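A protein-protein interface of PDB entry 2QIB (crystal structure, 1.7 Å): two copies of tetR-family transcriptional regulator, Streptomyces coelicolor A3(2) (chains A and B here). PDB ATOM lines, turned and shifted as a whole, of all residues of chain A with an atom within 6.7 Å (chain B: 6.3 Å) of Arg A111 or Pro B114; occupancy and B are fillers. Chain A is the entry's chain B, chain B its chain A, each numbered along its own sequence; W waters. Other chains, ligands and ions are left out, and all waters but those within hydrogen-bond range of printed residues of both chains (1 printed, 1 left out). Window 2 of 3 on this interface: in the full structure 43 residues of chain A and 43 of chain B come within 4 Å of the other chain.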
ATOM      1  N   PHE A 106      21.596   5.178  21.555  1.00  0.00           N
ATOM      2  CA  PHE A 106      21.947   4.587  22.866  1.00  0.00           C
ATOM      3  C   PHE A 106      20.726   4.661  23.792  1.00  0.00           C
ATOM      4  O   PHE A 106      20.316   3.660  24.365  1.00  0.00           O
ATOM      5  CB  PHE A 106      23.159   5.359  23.422  1.00  0.00           C
ATOM      6  CG  PHE A 106      23.703   4.843  24.728  1.00  0.00           C
ATOM      7  CD1 PHE A 106      24.568   3.753  24.766  1.00  0.00           C
ATOM      8  CD2 PHE A 106      23.446   5.527  25.899  1.00  0.00           C
ATOM      9  CE1 PHE A 106      25.105   3.316  25.999  1.00  0.00           C
ATOM     10  CE2 PHE A 106      23.969   5.083  27.137  1.00  0.00           C
ATOM     11  CZ  PHE A 106      24.781   4.000  27.185  1.00  0.00           C
ATOM     12  N   SER A 107      20.132   5.844  23.898  1.00  0.00           N
ATOM     13  CA  SER A 107      18.941   6.027  24.702  1.00  0.00           C
ATOM     14  C   SER A 107      17.829   5.081  24.282  1.00  0.00           C
ATOM     15  O   SER A 107      17.248   4.384  25.125  1.00  0.00           O
ATOM     16  CB  SER A 107      18.455   7.474  24.623  1.00  0.00           C
ATOM     17  OG  SER A 107      19.431   8.313  25.215  1.00  0.00           O
ATOM     18  N   ALA A 108      17.552   5.040  22.983  1.00  0.00           N
ATOM     19  CA  ALA A 108      16.478   4.187  22.497  1.00  0.00           C
ATOM     20  C   ALA A 108      16.752   2.697  22.743  1.00  0.00           C
ATOM     21  O   ALA A 108      15.827   1.957  23.106  1.00  0.00           O
ATOM     22  CB  ALA A 108      16.185   4.466  21.017  1.00  0.00           C
ATOM     23  N   LEU A 109      18.001   2.254  22.549  1.00  0.00           N
ATOM     24  CA  LEU A 109      18.363   0.853  22.775  1.00  0.00           C
ATOM     25  C   LEU A 109      18.190   0.460  24.228  1.00  0.00           C
ATOM     26  O   LEU A 109      17.533  -0.553  24.538  1.00  0.00           O
ATOM     27  CB  LEU A 109      19.806   0.569  22.312  1.00  0.00           C
ATOM     28  CG  LEU A 109      20.368  -0.828  22.577  1.00  0.00           C
ATOM     29  CD1 LEU A 109      19.625  -1.858  21.768  1.00  0.00           C
ATOM     30  CD2 LEU A 109      21.829  -0.863  22.278  1.00  0.00           C
ATOM     31  N   MET A 110      18.752   1.273  25.118  1.00  0.00           N
ATOM     32  CA  MET A 110      18.741   0.950  26.552  1.00  0.00           C
ATOM     33  C   MET A 110      17.332   1.033  27.155  1.00  0.00           C
ATOM     34  O   MET A 110      17.042   0.346  28.130  1.00  0.00           O
ATOM     35  CB  MET A 110      19.767   1.783  27.320  1.00  0.00           C
ATOM     36  CG  MET A 110      21.187   1.673  26.798  1.00  0.00           C
ATOM     37  SD  MET A 110      21.855  -0.177  26.468  1.00  0.00           S
ATOM     38  CE  MET A 110      23.535   0.303  25.650  1.00  0.00           C
ATOM     39  N   ARG A 111      16.453   1.828  26.549  1.00  0.00           N
ATOM     40  CA  ARG A 111      15.019   1.781  26.890  1.00  0.00           C
ATOM     41  C   ARG A 111      14.292   0.935  25.858  1.00  0.00           C
ATOM     42  O   ARG A 111      13.120   0.585  26.039  1.00  0.00           O
ATOM     43  CB  ARG A 111      14.403   3.183  26.952  1.00  0.00           C
ATOM     44  CG  ARG A 111      15.158   4.160  27.814  1.00  0.00           C
ATOM     45  CD  ARG A 111      14.589   5.583  27.729  1.00  0.00           C
ATOM     46  NE  ARG A 111      15.612   6.580  28.086  1.00  0.00           N
ATOM     47  CZ  ARG A 111      15.859   7.027  29.321  1.00  0.00           C
ATOM     48  NH1 ARG A 111      15.160   6.587  30.369  1.00  0.00           N
ATOM     49  NH2 ARG A 111      16.817   7.919  29.516  1.00  0.00           N
ATOM     50  N   ASN A 122      20.723  -7.949  22.836  1.00  0.00           N
ATOM     51  CA  ASN A 122      21.016  -8.181  24.272  1.00  0.00           C
ATOM     52  C   ASN A 122      22.384  -8.777  24.480  1.00  0.00           C
ATOM     53  O   ASN A 122      23.114  -8.368  25.397  1.00  0.00           O
ATOM     54  CB  ASN A 122      19.977  -9.099  24.922  1.00  0.00           C
ATOM     55  CG  ASN A 122      18.716  -8.367  25.305  1.00  0.00           C
ATOM     56  OD1 ASN A 122      18.602  -7.147  25.099  1.00  0.00           O
ATOM     57  ND2 ASN A 122      17.754  -9.095  25.889  1.00  0.00           N
ATOM     58  N   LEU A 165      22.965   7.345  30.742  1.00  0.00           N
ATOM     59  CA  LEU A 165      21.583   7.466  30.192  1.00  0.00           C
ATOM     60  C   LEU A 165      20.831   8.658  30.793  1.00  0.00           C
ATOM     61  O   LEU A 165      20.149   9.422  30.091  1.00  0.00           O
ATOM     62  CB  LEU A 165      20.826   6.162  30.470  1.00  0.00           C
ATOM     63  CG  LEU A 165      21.285   5.001  29.598  1.00  0.00           C
ATOM     64  CD1 LEU A 165      20.707   3.737  30.190  1.00  0.00           C
ATOM     65  CD2 LEU A 165      20.803   5.205  28.131  1.00  0.00           C
ATOM     66  N   LEU A 166      21.001   8.846  32.100  1.00  0.00           N
ATOM     67  CA  LEU A 166      20.386   9.959  32.793  1.00  0.00           C
ATOM     68  C   LEU A 166      21.014  11.281  32.314  1.00  0.00           C
ATOM     69  O   LEU A 166      20.305  12.294  32.161  1.00  0.00           O
ATOM     70  CB  LEU A 166      20.534   9.793  34.322  1.00  0.00           C
ATOM     71  CG  LEU A 166      19.724   8.597  34.841  1.00  0.00           C
ATOM     72  CD1 LEU A 166      20.205   8.243  36.258  1.00  0.00           C
ATOM     73  CD2 LEU A 166      18.203   8.857  34.829  1.00  0.00           C
ATOM     74  N   LEU A 168      22.139  12.002  29.359  1.00  0.00           N
ATOM     75  CA  LEU A 168      21.599  12.294  28.008  1.00  0.00           C
ATOM     76  C   LEU A 168      20.224  12.943  28.002  1.00  0.00           C
ATOM     77  O   LEU A 168      19.855  13.623  27.047  1.00  0.00           O
ATOM     78  CB  LEU A 168      21.525  11.026  27.196  1.00  0.00           C
ATOM     79  CG  LEU A 168      22.868  10.525  26.653  1.00  0.00           C
ATOM     80  CD1 LEU A 168      22.594   9.204  25.986  1.00  0.00           C
ATOM     81  CD2 LEU A 168      23.509  11.543  25.639  1.00  0.00           C
ATOM     82  N   ASP A 169      19.474  12.739  29.074  1.00  0.00           N
ATOM     83  CA  ASP A 169      18.147  13.376  29.197  1.00  0.00           C
ATOM     84  C   ASP A 169      18.238  14.828  29.672  1.00  0.00           C
ATOM     85  O   ASP A 169      17.913  15.146  30.825  1.00  0.00           O
ATOM     86  CB  ASP A 169      17.237  12.569  30.138  1.00  0.00           C
ATOM     87  CG  ASP A 169      15.745  12.965  30.001  1.00  0.00           C
ATOM     88  OD1 ASP A 169      15.429  13.916  29.238  1.00  0.00           O
ATOM     89  OD2 ASP A 169      14.895  12.303  30.643  1.00  0.00           O
ATOM     90  N   LEU B 109      13.122 -11.810  33.884  1.00  0.00           N
ATOM     91  CA  LEU B 109      12.517 -10.569  33.409  1.00  0.00           C
ATOM     92  C   LEU B 109      13.564  -9.478  33.257  1.00  0.00           C
ATOM     93  O   LEU B 109      13.592  -8.765  32.249  1.00  0.00           O
ATOM     94  CB  LEU B 109      11.435 -10.085  34.366  1.00  0.00           C
ATOM     95  CG  LEU B 109      10.759  -8.745  34.072  1.00  0.00           C
ATOM     96  CD1 LEU B 109       9.960  -8.810  32.781  1.00  0.00           C
ATOM     97  CD2 LEU B 109       9.895  -8.335  35.215  1.00  0.00           C
ATOM     98  N   MET B 110      14.411  -9.351  34.269  1.00  0.00           N
ATOM     99  CA  MET B 110      15.343  -8.223  34.302  1.00  0.00           C
ATOM    100  C   MET B 110      16.499  -8.444  33.342  1.00  0.00           C
ATOM    101  O   MET B 110      16.941  -7.500  32.679  1.00  0.00           O
ATOM    102  CB  MET B 110      15.833  -7.936  35.724  1.00  0.00           C
ATOM    103  CG  MET B 110      14.732  -7.603  36.713  1.00  0.00           C
ATOM    104  SD  MET B 110      13.447  -6.176  36.158  1.00  0.00           S
ATOM    105  CE  MET B 110      14.672  -4.653  36.215  1.00  0.00           C
ATOM    106  N   GLY B 112      16.407 -10.212  30.656  1.00  0.00           N
ATOM    107  CA  GLY B 112      15.789  -9.958  29.350  1.00  0.00           C
ATOM    108  C   GLY B 112      15.790  -8.468  28.995  1.00  0.00           C
ATOM    109  O   GLY B 112      16.151  -8.098  27.882  1.00  0.00           O
ATOM    110  N   GLY B 113      15.396  -7.604  29.930  1.00  0.00           N
ATOM    111  CA  GLY B 113      15.369  -6.148  29.680  1.00  0.00           C
ATOM    112  C   GLY B 113      14.181  -5.673  28.838  1.00  0.00           C
ATOM    113  O   GLY B 113      13.287  -6.474  28.516  1.00  0.00           O
ATOM    114  N   PRO B 114      14.166  -4.374  28.461  1.00  0.00           N
ATOM    115  CA  PRO B 114      13.126  -3.777  27.598  1.00  0.00           C
ATOM    116  C   PRO B 114      13.003  -4.372  26.177  1.00  0.00           C
ATOM    117  O   PRO B 114      11.926  -4.310  25.578  1.00  0.00           O
ATOM    118  CB  PRO B 114      13.542  -2.299  27.513  1.00  0.00           C
ATOM    119  CG  PRO B 114      15.010  -2.290  27.821  1.00  0.00           C
ATOM    120  CD  PRO B 114      15.174  -3.371  28.865  1.00  0.00           C
ATOM    121  N   ALA B 115      14.081  -4.937  25.637  1.00  0.00           N
ATOM    122  CA  ALA B 115      14.009  -5.534  24.298  1.00  0.00           C
ATOM    123  C   ALA B 115      13.049  -6.738  24.242  1.00  0.00           C
ATOM    124  O   ALA B 115      12.220  -6.830  23.346  1.00  0.00           O
ATOM    125  CB  ALA B 115      15.413  -5.907  23.786  1.00  0.00           C
ATOM    126  N   VAL B 116      13.162  -7.640  25.215  1.00  0.00           N
ATOM    127  CA  VAL B 116      12.331  -8.842  25.298  1.00  0.00           C
ATOM    128  C   VAL B 116      10.934  -8.469  25.814  1.00  0.00           C
ATOM    129  O   VAL B 116       9.918  -9.012  25.347  1.00  0.00           O
ATOM    130  CB  VAL B 116      12.988  -9.953  26.210  1.00  0.00           C
ATOM    131  CG1 VAL B 116      12.007 -11.108  26.498  1.00  0.00           C
ATOM    132  CG2 VAL B 116      14.270 -10.499  25.578  1.00  0.00           C
ATOM    133  N   GLY B 117      10.884  -7.527  26.756  1.00  0.00           N
ATOM    134  CA  GLY B 117       9.620  -7.157  27.381  1.00  0.00           C
ATOM    135  C   GLY B 117       8.609  -6.591  26.400  1.00  0.00           C
ATOM    136  O   GLY B 117       8.986  -5.932  25.425  1.00  0.00           O
ATOM    137  N   SER B 118       7.325  -6.857  26.641  1.00  0.00           N
ATOM    138  CA  SER B 118       6.279  -6.186  25.887  1.00  0.00           C
ATOM    139  C   SER B 118       6.256  -4.739  26.356  1.00  0.00           C
ATOM    140  O   SER B 118       6.869  -4.390  27.385  1.00  0.00           O
ATOM    141  CB  SER B 118       4.917  -6.827  26.116  1.00  0.00           C
ATOM    142  OG  SER B 118       4.518  -6.694  27.460  1.00  0.00           O
ATOM    143  N   ASN B 122       7.441  -3.644  30.145  1.00  0.00           N
ATOM    144  CA  ASN B 122       8.385  -2.513  30.356  1.00  0.00           C
ATOM    145  C   ASN B 122       7.787  -1.363  31.127  1.00  0.00           C
ATOM    146  O   ASN B 122       8.473  -0.766  31.972  1.00  0.00           O
ATOM    147  CB  ASN B 122       8.923  -1.976  29.033  1.00  0.00           C
ATOM    148  CG  ASN B 122       9.662  -3.019  28.266  1.00  0.00           C
ATOM    149  OD1 ASN B 122      10.048  -4.050  28.829  1.00  0.00           O
ATOM    150  ND2 ASN B 122       9.833  -2.795  26.955  1.00  0.00           N
ATOM    151  N   ARG B 129      10.045   1.310  39.325  1.00  0.00           N
ATOM    152  CA  ARG B 129      11.195   2.199  39.481  1.00  0.00           C
ATOM    153  C   ARG B 129      10.739   3.600  39.871  1.00  0.00           C
ATOM    154  O   ARG B 129      11.307   4.219  40.787  1.00  0.00           O
ATOM    155  CB  ARG B 129      11.994   2.265  38.187  1.00  0.00           C
ATOM    156  CG  ARG B 129      12.657   0.954  37.846  1.00  0.00           C
ATOM    157  CD  ARG B 129      13.297   1.068  36.462  1.00  0.00           C
ATOM    158  NE  ARG B 129      14.064  -0.130  36.161  1.00  0.00           N
ATOM    159  CZ  ARG B 129      14.098  -0.706  34.979  1.00  0.00           C
ATOM    160  NH1 ARG B 129      13.352  -0.213  33.973  1.00  0.00           N
ATOM    161  NH2 ARG B 129      14.823  -1.806  34.814  1.00  0.00           N
HETATM  162  O   HOH W   1      16.829  -4.972  26.729  1.00  0.00           O
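ND2 of Asn A122 is in hydrogen-bond range of O of Gly B112 (2.7 Å).
O of Pro B114 lies within hydrogen-bond range of ND2 of Asn B122 (2.9 Å).
Among the printed residues, merely in contact across the chains: Arg A111 with Pro B114, Met A110 with Pro B114, Asn A122 with Ala B115 and Asn A122 with Val B116.
Of chain A, only Met A110 and Arg A111 come within 4 Å of Pro B114.
Of the printed residues of chain A, Gly B112 touches Asn A122.
Printed residues of chain B within 4 Å of Met A110: Pro B114.
Printed residues of chain A within 4 Å of Ala B115: Asn A122 (3.7 Å).
Of the printed residues of chain A, Val B116 touches Asn A122 (3.8 Å).
Of the printed residues of chain B, Asn A122 touches Gly B112 (2.7 Å), Ala B115 (3.7 Å) and Val B116 (3.8 Å).
Asn B122 touches none of the printed residues of chain A.
Ser B118 touches none of the printed residues of chain A.
The nearest printed residue of chain B that does not touch Asn A122 is Gly B113 (4.9 Å).
Among the printed residues, no Asp or Glu carboxylate lies within 4 Å of a Lys or Arg side-chain nitrogen of the other chain.
Positions printed for both chains: 109, 110 and 122.
Water W1 lies within hydrogen-bond range of the backbone NH (N) of Ala B115, the side-chain amide oxygen (OD1) of Asn A122 and the backbone carbonyl oxygen (O) of Gly B112.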
